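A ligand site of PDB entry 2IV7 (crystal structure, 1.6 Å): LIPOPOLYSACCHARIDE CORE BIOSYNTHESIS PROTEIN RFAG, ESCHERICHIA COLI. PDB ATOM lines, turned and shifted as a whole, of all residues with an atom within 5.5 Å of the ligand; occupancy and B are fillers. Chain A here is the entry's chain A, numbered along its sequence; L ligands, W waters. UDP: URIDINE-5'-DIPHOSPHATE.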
ATOM      1  N   PRO A  12     -22.451  33.255  21.533  1.00  0.00           N
ATOM      2  CA  PRO A  12     -22.934  31.878  21.434  1.00  0.00           C
ATOM      3  C   PRO A  12     -22.702  31.126  20.119  1.00  0.00           C
ATOM      4  O   PRO A  12     -22.944  29.904  20.068  1.00  0.00           O
ATOM      5  CB  PRO A  12     -24.451  32.021  21.677  1.00  0.00           C
ATOM      6  CG  PRO A  12     -24.623  33.408  22.244  1.00  0.00           C
ATOM      7  CD  PRO A  12     -23.545  34.227  21.611  1.00  0.00           C
ATOM      8  N   PHE A  13     -22.235  31.816  19.090  1.00  0.00           N
ATOM      9  CA  PHE A  13     -22.261  31.255  17.735  1.00  0.00           C
ATOM     10  C   PHE A  13     -20.894  30.962  17.130  1.00  0.00           C
ATOM     11  O   PHE A  13     -20.703  31.035  15.910  1.00  0.00           O
ATOM     12  CB  PHE A  13     -23.085  32.169  16.818  1.00  0.00           C
ATOM     13  CG  PHE A  13     -24.411  32.546  17.419  1.00  0.00           C
ATOM     14  CD1 PHE A  13     -25.366  31.574  17.711  1.00  0.00           C
ATOM     15  CD2 PHE A  13     -24.692  33.890  17.726  1.00  0.00           C
ATOM     16  CE1 PHE A  13     -26.609  31.923  18.276  1.00  0.00           C
ATOM     17  CE2 PHE A  13     -25.930  34.240  18.304  1.00  0.00           C
ATOM     18  CZ  PHE A  13     -26.887  33.246  18.575  1.00  0.00           C
ATOM     19  N   GLY A  14     -19.963  30.591  18.000  1.00  0.00           N
ATOM     20  CA  GLY A  14     -18.604  30.234  17.590  1.00  0.00           C
ATOM     21  C   GLY A  14     -18.163  28.937  18.233  1.00  0.00           C
ATOM     22  O   GLY A  14     -18.543  28.636  19.372  1.00  0.00           O
ATOM     23  N   GLY A  15     -17.358  28.154  17.507  1.00  0.00           N
ATOM     24  CA  GLY A  15     -16.909  26.846  17.989  1.00  0.00           C
ATOM     25  C   GLY A  15     -16.008  26.945  19.214  1.00  0.00           C
ATOM     26  O   GLY A  15     -16.197  26.206  20.181  1.00  0.00           O
ATOM     27  N   LEU A  16     -15.017  27.819  19.147  1.00  0.00           N
ATOM     28  CA  LEU A  16     -14.140  28.062  20.300  1.00  0.00           C
ATOM     29  C   LEU A  16     -14.979  28.332  21.548  1.00  0.00           C
ATOM     30  O   LEU A  16     -14.760  27.758  22.636  1.00  0.00           O
ATOM     31  CB  LEU A  16     -13.207  29.242  19.985  1.00  0.00           C
ATOM     32  CG  LEU A  16     -12.207  29.751  21.014  1.00  0.00           C
ATOM     33  CD1 LEU A  16     -11.235  30.669  20.318  1.00  0.00           C
ATOM     34  CD2 LEU A  16     -12.880  30.463  22.184  1.00  0.00           C
ATOM     35  N   ARG A  18     -18.249  27.697  22.106  1.00  0.00           N
ATOM     36  CA  ARG A  18     -19.103  26.583  22.533  1.00  0.00           C
ATOM     37  C   ARG A  18     -18.313  25.462  23.206  1.00  0.00           C
ATOM     38  O   ARG A  18     -18.792  24.832  24.161  1.00  0.00           O
ATOM     39  CG  ARG A  18     -21.083  27.068  21.048  1.00  0.00           C
ATOM     40  CD  ARG A  18     -21.961  26.643  19.880  1.00  0.00           C
ATOM     41  NE  ARG A  18     -22.451  25.268  19.964  1.00  0.00           N
ATOM     42  CZ  ARG A  18     -23.672  24.904  20.323  1.00  0.00           C
ATOM     43  NH1 ARG A  18     -24.574  25.815  20.657  1.00  0.00           N
ATOM     44  NH2 ARG A  18     -24.006  23.617  20.331  1.00  0.00           N
ATOM     45  N   ARG A 173     -27.931  18.020  18.974  1.00  0.00           N
ATOM     46  CA  ARG A 173     -27.937  17.939  17.502  1.00  0.00           C
ATOM     47  C   ARG A 173     -28.297  16.553  16.958  1.00  0.00           C
ATOM     48  O   ARG A 173     -28.653  16.417  15.775  1.00  0.00           O
ATOM     49  CB  ARG A 173     -26.597  18.355  16.909  1.00  0.00           C
ATOM     50  CG  ARG A 173     -26.410  19.844  16.781  1.00  0.00           C
ATOM     51  CD  ARG A 173     -25.901  20.482  18.069  1.00  0.00           C
ATOM     52  NE  ARG A 173     -25.483  21.857  17.763  1.00  0.00           N
ATOM     53  CZ  ARG A 173     -26.266  22.934  17.774  1.00  0.00           C
ATOM     54  NH1 ARG A 173     -27.544  22.846  18.158  1.00  0.00           N
ATOM     55  NH2 ARG A 173     -25.756  24.109  17.420  1.00  0.00           N
ATOM     56  N   VAL A 202     -23.668  26.538   7.898  1.00  0.00           N
ATOM     57  CA  VAL A 202     -23.689  27.138   9.247  1.00  0.00           C
ATOM     58  C   VAL A 202     -22.276  27.502   9.655  1.00  0.00           C
ATOM     59  O   VAL A 202     -21.357  26.700   9.536  1.00  0.00           O
ATOM     60  CB  VAL A 202     -24.275  26.146  10.294  1.00  0.00           C
ATOM     61  CG1 VAL A 202     -24.144  26.700  11.716  1.00  0.00           C
ATOM     62  CG2 VAL A 202     -25.723  25.826   9.972  1.00  0.00           C
ATOM     63  N   GLY A 203     -22.112  28.740  10.126  1.00  0.00           N
ATOM     64  CA  GLY A 203     -20.811  29.210  10.608  1.00  0.00           C
ATOM     65  C   GLY A 203     -20.679  30.717  10.553  1.00  0.00           C
ATOM     66  O   GLY A 203     -21.119  31.351   9.596  1.00  0.00           O
ATOM     67  N   SER A 204     -20.016  31.286  11.553  1.00  0.00           N
ATOM     68  CA  SER A 204     -19.954  32.735  11.706  1.00  0.00           C
ATOM     69  C   SER A 204     -18.752  33.405  11.026  1.00  0.00           C
ATOM     70  O   SER A 204     -18.256  34.436  11.489  1.00  0.00           O
ATOM     71  CB  SER A 204     -20.014  33.089  13.207  1.00  0.00           C
ATOM     72  OG  SER A 204     -21.267  32.706  13.759  1.00  0.00           O
ATOM     73  N   ARG A 208     -14.353  32.806   5.132  1.00  0.00           N
ATOM     74  CA  ARG A 208     -13.427  31.733   5.444  1.00  0.00           C
ATOM     75  C   ARG A 208     -14.062  30.373   5.129  1.00  0.00           C
ATOM     76  O   ARG A 208     -13.384  29.446   4.689  1.00  0.00           O
ATOM     77  CB  ARG A 208     -13.045  31.809   6.914  1.00  0.00           C
ATOM     78  CG  ARG A 208     -12.181  30.642   7.313  1.00  0.00           C
ATOM     79  CD  ARG A 208     -11.560  30.852   8.667  1.00  0.00           C
ATOM     80  NE  ARG A 208     -12.517  31.049   9.758  1.00  0.00           N
ATOM     81  CZ  ARG A 208     -13.148  30.081  10.414  1.00  0.00           C
ATOM     82  NH1 ARG A 208     -12.970  28.808  10.059  1.00  0.00           N
ATOM     83  NH2 ARG A 208     -13.960  30.387  11.410  1.00  0.00           N
ATOM     84  N   LYS A 209     -15.367  30.279   5.349  1.00  0.00           N
ATOM     85  CA  LYS A 209     -16.058  29.003   5.239  1.00  0.00           C
ATOM     86  C   LYS A 209     -16.587  28.710   3.832  1.00  0.00           C
ATOM     87  O   LYS A 209     -17.241  27.698   3.608  1.00  0.00           O
ATOM     88  CB  LYS A 209     -17.135  28.885   6.304  1.00  0.00           C
ATOM     89  CG  LYS A 209     -16.527  28.824   7.719  1.00  0.00           C
ATOM     90  CD  LYS A 209     -17.610  29.020   8.766  1.00  0.00           C
ATOM     91  CE  LYS A 209     -16.987  29.118  10.161  1.00  0.00           C
ATOM     92  NZ  LYS A 209     -16.541  27.766  10.631  1.00  0.00           N
ATOM     93  N   VAL A 234     -26.226  30.639   7.614  1.00  0.00           N
ATOM     94  CA  VAL A 234     -26.551  30.984   8.994  1.00  0.00           C
ATOM     95  C   VAL A 234     -25.284  31.282   9.783  1.00  0.00           C
ATOM     96  O   VAL A 234     -24.404  30.406   9.886  1.00  0.00           O
ATOM     97  CB  VAL A 234     -27.293  29.818   9.676  1.00  0.00           C
ATOM     98  CG1 VAL A 234     -27.561  30.164  11.148  1.00  0.00           C
ATOM     99  CG2 VAL A 234     -28.591  29.486   8.953  1.00  0.00           C
ATOM    100  N   GLY A 235     -25.187  32.482  10.341  1.00  0.00           N
ATOM    101  CA  GLY A 235     -24.068  32.817  11.235  1.00  0.00           C
ATOM    102  C   GLY A 235     -23.986  34.282  11.569  1.00  0.00           C
ATOM    103  O   GLY A 235     -24.603  35.111  10.904  1.00  0.00           O
ATOM    104  N   GLN A 236     -23.207  34.572  12.613  1.00  0.00           N
ATOM    105  CA  GLN A 236     -22.990  35.950  13.036  1.00  0.00           C
ATOM    106  C   GLN A 236     -21.880  36.585  12.173  1.00  0.00           C
ATOM    107  O   GLN A 236     -20.712  36.660  12.569  1.00  0.00           O
ATOM    108  CB  GLN A 236     -22.643  36.023  14.527  1.00  0.00           C
ATOM    109  CG  GLN A 236     -22.567  37.470  15.037  1.00  0.00           C
ATOM    110  CD  GLN A 236     -22.645  37.556  16.556  1.00  0.00           C
ATOM    111  OE1 GLN A 236     -23.570  37.027  17.166  1.00  0.00           O
ATOM    112  NE2 GLN A 236     -21.667  38.235  17.156  1.00  0.00           N
ATOM    113  N   SER A 259     -28.611  35.848  10.729  1.00  0.00           N
ATOM    114  CA  SER A 259     -27.614  36.106  11.770  1.00  0.00           C
ATOM    115  C   SER A 259     -27.455  34.829  12.591  1.00  0.00           C
ATOM    116  O   SER A 259     -27.968  33.767  12.204  1.00  0.00           O
ATOM    117  CB  SER A 259     -28.086  37.267  12.636  1.00  0.00           C
ATOM    118  OG  SER A 259     -28.162  38.440  11.841  1.00  0.00           O
ATOM    119  N   GLY A 260     -26.728  34.903  13.715  1.00  0.00           N
ATOM    120  CA  GLY A 260     -26.551  33.731  14.571  1.00  0.00           C
ATOM    121  C   GLY A 260     -27.881  33.146  14.978  1.00  0.00           C
ATOM    122  O   GLY A 260     -28.769  33.887  15.397  1.00  0.00           O
ATOM    123  N   ARG A 261     -28.028  31.821  14.837  1.00  0.00           N
ATOM    124  CA  ARG A 261     -29.241  31.113  15.228  1.00  0.00           C
ATOM    125  C   ARG A 261     -28.988  30.050  16.308  1.00  0.00           C
ATOM    126  O   ARG A 261     -27.969  29.358  16.269  1.00  0.00           O
ATOM    127  CB  ARG A 261     -29.940  30.495  14.009  1.00  0.00           C
ATOM    128  CG  ARG A 261     -30.609  31.557  13.113  1.00  0.00           C
ATOM    129  CD  ARG A 261     -31.258  30.961  11.867  1.00  0.00           C
ATOM    130  NE  ARG A 261     -32.423  30.140  12.155  1.00  0.00           N
ATOM    131  CZ  ARG A 261     -33.381  29.853  11.283  1.00  0.00           C
ATOM    132  NH1 ARG A 261     -33.302  30.330  10.036  1.00  0.00           N
ATOM    133  NH2 ARG A 261     -34.405  29.093  11.637  1.00  0.00           N
ATOM    134  N   ASN A 262     -29.940  29.914  17.222  1.00  0.00           N
ATOM    135  CA  ASN A 262     -29.896  28.937  18.308  1.00  0.00           C
ATOM    136  C   ASN A 262     -30.644  27.643  17.978  1.00  0.00           C
ATOM    137  O   ASN A 262     -30.741  26.730  18.827  1.00  0.00           O
ATOM    138  CB  ASN A 262     -30.470  29.543  19.604  1.00  0.00           C
ATOM    139  CG  ASN A 262     -29.706  30.761  20.066  1.00  0.00           C
ATOM    140  OD1 ASN A 262     -28.545  30.674  20.441  1.00  0.00           O
ATOM    141  ND2 ASN A 262     -30.385  31.908  20.082  1.00  0.00           N
ATOM    142  N   VAL A 264     -29.950  25.576  15.226  1.00  0.00           N
ATOM    143  CA  VAL A 264     -29.202  24.779  14.220  1.00  0.00           C
ATOM    144  C   VAL A 264     -29.582  23.284  14.216  1.00  0.00           C
ATOM    145  O   VAL A 264     -29.658  22.659  13.145  1.00  0.00           O
ATOM    146  CB  VAL A 264     -27.676  25.005  14.358  1.00  0.00           C
ATOM    147  CG1 VAL A 264     -26.880  24.007  13.509  1.00  0.00           C
ATOM    148  CG2 VAL A 264     -27.307  26.447  13.947  1.00  0.00           C
ATOM    149  N   MET A 268     -30.756  21.353  10.864  1.00  0.00           N
ATOM    150  CA  MET A 268     -30.117  20.141  10.375  1.00  0.00           C
ATOM    151  C   MET A 268     -31.101  18.990  10.195  1.00  0.00           C
ATOM    152  O   MET A 268     -30.930  18.169   9.312  1.00  0.00           O
ATOM    153  CB  MET A 268     -28.922  19.750  11.255  1.00  0.00           C
ATOM    154  CG  MET A 268     -27.788  20.757  11.167  1.00  0.00           C
ATOM    155  SD  MET A 268     -26.275  20.119  12.181  1.00  0.00           S
ATOM    156  CE  MET A 268     -24.991  21.491  11.624  1.00  0.00           C
ATOM    157  N   HIS A 276     -20.234  22.854   3.281  1.00  0.00           N
ATOM    158  CA  HIS A 276     -19.190  23.527   4.053  1.00  0.00           C
ATOM    159  C   HIS A 276     -17.852  23.519   3.319  1.00  0.00           C
ATOM    160  O   HIS A 276     -16.880  22.918   3.777  1.00  0.00           O
ATOM    161  CB  HIS A 276     -19.058  22.863   5.426  1.00  0.00           C
ATOM    162  CG  HIS A 276     -18.444  23.762   6.454  1.00  0.00           C
ATOM    163  ND1 HIS A 276     -17.107  23.709   6.793  1.00  0.00           N
ATOM    164  CD2 HIS A 276     -18.993  24.750   7.190  1.00  0.00           C
ATOM    165  CE1 HIS A 276     -16.861  24.635   7.714  1.00  0.00           C
ATOM    166  NE2 HIS A 276     -17.990  25.272   7.976  1.00  0.00           N
ATOM    167  N   GLU A 281     -10.210  25.737   8.139  1.00  0.00           N
ATOM    168  CA  GLU A 281     -11.017  25.234   9.225  1.00  0.00           C
ATOM    169  C   GLU A 281     -10.174  24.293  10.083  1.00  0.00           C
ATOM    170  O   GLU A 281      -9.821  23.210   9.634  1.00  0.00           O
ATOM    171  CB  GLU A 281     -12.244  24.487   8.674  1.00  0.00           C
ATOM    172  CG  GLU A 281     -13.356  24.291   9.679  1.00  0.00           C
ATOM    173  CD  GLU A 281     -14.065  25.588  10.017  1.00  0.00           C
ATOM    174  OE1 GLU A 281     -14.960  25.992   9.237  1.00  0.00           O
ATOM    175  OE2 GLU A 281     -13.708  26.209  11.037  1.00  0.00           O
ATOM    176  N   ALA A 283     -10.961  22.565  12.651  1.00  0.00           N
ATOM    177  CA  ALA A 283     -11.685  21.326  12.891  1.00  0.00           C
ATOM    178  C   ALA A 283     -13.000  21.351  12.123  1.00  0.00           C
ATOM    179  O   ALA A 283     -13.078  20.768  11.051  1.00  0.00           O
ATOM    180  CB  ALA A 283     -11.889  21.087  14.393  1.00  0.00           C
ATOM    181  N   GLY A 284     -14.005  22.057  12.646  1.00  0.00           N
ATOM    182  CA  GLY A 284     -15.279  22.197  11.956  1.00  0.00           C
ATOM    183  C   GLY A 284     -16.344  21.365  12.645  1.00  0.00           C
ATOM    184  O   GLY A 284     -16.766  20.303  12.148  1.00  0.00           O
ATOM    185  N   ILE A 285     -16.790  21.850  13.808  1.00  0.00           N
ATOM    186  CA  ILE A 285     -17.843  21.213  14.583  1.00  0.00           C
ATOM    187  C   ILE A 285     -19.083  20.933  13.731  1.00  0.00           C
ATOM    188  O   ILE A 285     -19.677  19.866  13.856  1.00  0.00           O
ATOM    189  CB  ILE A 285     -18.209  22.058  15.845  1.00  0.00           C
ATOM    190  CG1 ILE A 285     -17.016  22.131  16.798  1.00  0.00           C
ATOM    191  CG2 ILE A 285     -19.447  21.494  16.565  1.00  0.00           C
ATOM    192  CD1 ILE A 285     -17.142  23.217  17.849  1.00  0.00           C
ATOM    193  N   VAL A 286     -19.455  21.880  12.865  1.00  0.00           N
ATOM    194  CA  VAL A 286     -20.679  21.673  12.080  1.00  0.00           C
ATOM    195  C   VAL A 286     -20.641  20.407  11.218  1.00  0.00           C
ATOM    196  O   VAL A 286     -21.680  19.801  10.977  1.00  0.00           O
ATOM    197  CB  VAL A 286     -21.059  22.888  11.214  1.00  0.00           C
ATOM    198  CG1 VAL A 286     -21.425  24.068  12.109  1.00  0.00           C
ATOM    199  CG2 VAL A 286     -19.952  23.231  10.189  1.00  0.00           C
ATOM    200  N   LEU A 287     -19.438  20.002  10.799  1.00  0.00           N
ATOM    201  CA  LEU A 287     -19.322  18.789  10.005  1.00  0.00           C
ATOM    202  C   LEU A 287     -19.801  17.569  10.788  1.00  0.00           C
ATOM    203  O   LEU A 287     -20.541  16.727  10.257  1.00  0.00           O
ATOM    204  CB  LEU A 287     -17.874  18.565   9.579  1.00  0.00           C
ATOM    205  CG  LEU A 287     -17.265  19.683   8.745  1.00  0.00           C
ATOM    206  CD1 LEU A 287     -15.771  19.388   8.501  1.00  0.00           C
ATOM    207  CD2 LEU A 287     -18.023  19.867   7.433  1.00  0.00           C
ATOM    208  N   GLU A 289     -21.627  17.720  13.663  1.00  0.00           N
ATOM    209  CA  GLU A 289     -23.028  17.930  14.028  1.00  0.00           C
ATOM    210  C   GLU A 289     -23.931  17.355  12.943  1.00  0.00           C
ATOM    211  O   GLU A 289     -24.911  16.676  13.240  1.00  0.00           O
ATOM    212  CB  GLU A 289     -23.317  19.402  14.234  1.00  0.00           C
ATOM    213  CG  GLU A 289     -22.705  19.972  15.510  1.00  0.00           C
ATOM    214  CD  GLU A 289     -22.921  21.481  15.643  1.00  0.00           C
ATOM    215  OE1 GLU A 289     -23.113  22.168  14.623  1.00  0.00           O
ATOM    216  OE2 GLU A 289     -22.865  21.973  16.794  1.00  0.00           O
HETATM  217  N1  UDP L   1     -23.368  27.783  15.580  1.00  0.00           N
HETATM  218  C2  UDP L   1     -24.678  28.016  15.970  1.00  0.00           C
HETATM  219  N3  UDP L   1     -25.412  29.016  15.356  1.00  0.00           N
HETATM  220  C4  UDP L   1     -24.816  29.787  14.375  1.00  0.00           C
HETATM  221  C5  UDP L   1     -23.496  29.571  13.996  1.00  0.00           C
HETATM  222  C6  UDP L   1     -22.757  28.579  14.630  1.00  0.00           C
HETATM  223  O2  UDP L   1     -25.220  27.344  16.845  1.00  0.00           O
HETATM  224  O4  UDP L   1     -25.478  30.691  13.852  1.00  0.00           O
HETATM  225  C1' UDP L   1     -22.611  26.721  16.241  1.00  0.00           C
HETATM  226  C2' UDP L   1     -22.436  25.507  15.342  1.00  0.00           C
HETATM  227  O2' UDP L   1     -23.591  24.667  15.349  1.00  0.00           O
HETATM  228  C3' UDP L   1     -21.193  24.880  15.942  1.00  0.00           C
HETATM  229  C4' UDP L   1     -20.356  26.109  16.287  1.00  0.00           C
HETATM  230  O4' UDP L   1     -21.292  27.166  16.461  1.00  0.00           O
HETATM  231  O3' UDP L   1     -21.525  24.202  17.132  1.00  0.00           O
HETATM  232  C5' UDP L   1     -19.382  26.502  15.181  1.00  0.00           C
HETATM  233  O5' UDP L   1     -18.216  25.714  15.311  1.00  0.00           O
HETATM  234  PA  UDP L   1     -17.348  25.343  14.033  1.00  0.00           P
HETATM  235  O1A UDP L   1     -18.211  24.688  12.997  1.00  0.00           O
HETATM  236  O2A UDP L   1     -16.220  24.484  14.481  1.00  0.00           O
HETATM  237  O3A UDP L   1     -16.881  26.728  13.399  1.00  0.00           O
HETATM  238  PB  UDP L   1     -16.088  27.953  14.122  1.00  0.00           P
HETATM  239  O1B UDP L   1     -15.227  27.434  15.220  1.00  0.00           O
HETATM  240  O2B UDP L   1     -17.090  28.894  14.649  1.00  0.00           O
HETATM  241  O3B UDP L   1     -15.263  28.512  13.034  1.00  0.00           O
HETATM  242  O   HOH W   1     -12.548  25.755  16.035  1.00  0.00           O
HETATM  243  O   HOH W   2     -13.915  23.386  15.727  1.00  0.00           O
HETATM  244  O   HOH W   3     -27.874  26.318  17.456  1.00  0.00           O
HETATM  245  O   HOH W   4     -20.545  23.102  19.635  1.00  0.00           O
HETATM  246  O   HOH W   5     -19.611  29.613  13.807  1.00  0.00           O
HETATM  247  O   HOH W   6     -12.521  28.119  13.767  1.00  0.00           O
HETATM  248  O   HOH W   7     -13.979  29.158  16.721  1.00  0.00           O
HETATM  249  O   HOH W   8     -16.687  31.675  14.904  1.00  0.00           O
HETATM  250  O   HOH W   9     -19.026  26.521  11.090  1.00  0.00           O
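OE2 of Glu 289 is in salt-bridge range of NE of Arg 173, at 2.8 Å.
The guanidinium group (NH1) of Arg 208 lies within salt-bridge range of the side-chain carboxylate (OE2) of Glu 281 (2.9 Å).
The side-chain amino group of Lys 209 is in salt-bridge range of the side-chain carboxylate of Glu 281 (2.8 Å).
A ring nitrogen (NE2) of His 276 sits close to the side-chain carboxylate (OE1) of Glu 281, 3.4 Å away.
O of Phe 13 is in hydrogen-bond range of OG of Ser 204 (2.8 Å).
The backbone NH of Gly 203 is in hydrogen-bond range of the backbone carbonyl oxygen of Val 234 (2.8 Å).
OG of Ser 204 lies within hydrogen-bond range of N of Gln 236, 2.9 Å away.
OE2 of Glu 281 sits close to O3B of the ligand, 3.4 Å away.
Phe 13 touches the ligand.
CA of Gly 14 touches O2B of the ligand, at 3.6 Å.
N of Leu 16 touches O1B of the ligand (3.95 Å).
Val 202 touches the ligand (CG1 to C5, 3.7 Å).
Ser 204 touches the ligand.
Val 234 touches the ligand (CG1 to O4, 3.5 Å).
Gly 235 touches the ligand.
Gly 260 touches the ligand.
CG2 of Val 264 touches N3 of the ligand (3.5 Å).
Gly 284 touches the ligand (CA to O2A, 3.5 Å).
Hydrophobic or aromatic side chains that line the ligand: Phe 13, Val 202, Val 234, Val 264, Ile 285 and Val 286.
Of the 29 residues printed, 20 come within 4 Å of the ligand.
The nearest printed residue that does not touch the ligand is Gly 203 (4.2 Å).
Water W7 bridges an oxygen (O1B) of the ligand (2.6 Å) and the backbone NH (N) of Leu 16 (3.0 Å).
Water W5 lies within hydrogen-bond range of an oxygen (O2B) of the ligand, the backbone carbonyl oxygen (O) of Phe 13 and the backbone NH (N) of Ser 204.
Water W9 lies within hydrogen-bond range of an oxygen (O1A) of the ligand (2.8 Å), the backbone carbonyl oxygen of Val 202 (2.8 Å) and the side-chain amino group of Lys 209 (2.8 Å).
Water W2 lies within hydrogen-bond range of O2A of the ligand (2.8 Å) and N of Gly 284 (3.4 Å).
Water W4 bridges O3' of the ligand (2.9 Å) and NE of Arg 18 (2.9 Å).
The side-chain carboxylate (OE2) of Glu 289 sits at hydrogen-bond distance from an oxygen (O3') of the ligand.
O4 of the ligand lies within hydrogen-bond range of N of Arg 261.
N3 of the ligand is in hydrogen-bond range of O of Arg 261 (2.7 Å).
The backbone NH (N) of Ile 285 is in hydrogen-bond range of an oxygen (O2A) of the ligand (2.8 Å).
The guanidinium group (NH2) of Arg 208 is in salt-bridge range of an oxygen (O3B) of the ligand.
NZ of Lys 209 is in salt-bridge range of O3B of the ligand (2.8 Å).
N of Gly 15 is in hydrogen-bond range of O2B of the ligand, 3.0 Å away.
The guanidinium group of Arg 173 lies within hydrogen-bond range of an oxygen (O2') of the ligand (3.0 Å).
N of Val 286 sits at hydrogen-bond distance from O1A of the ligand (3.1 Å).
An oxygen (O3') of the ligand lies within hydrogen-bond range of the guanidinium group (NE) of Arg 18, 3.2 Å away.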
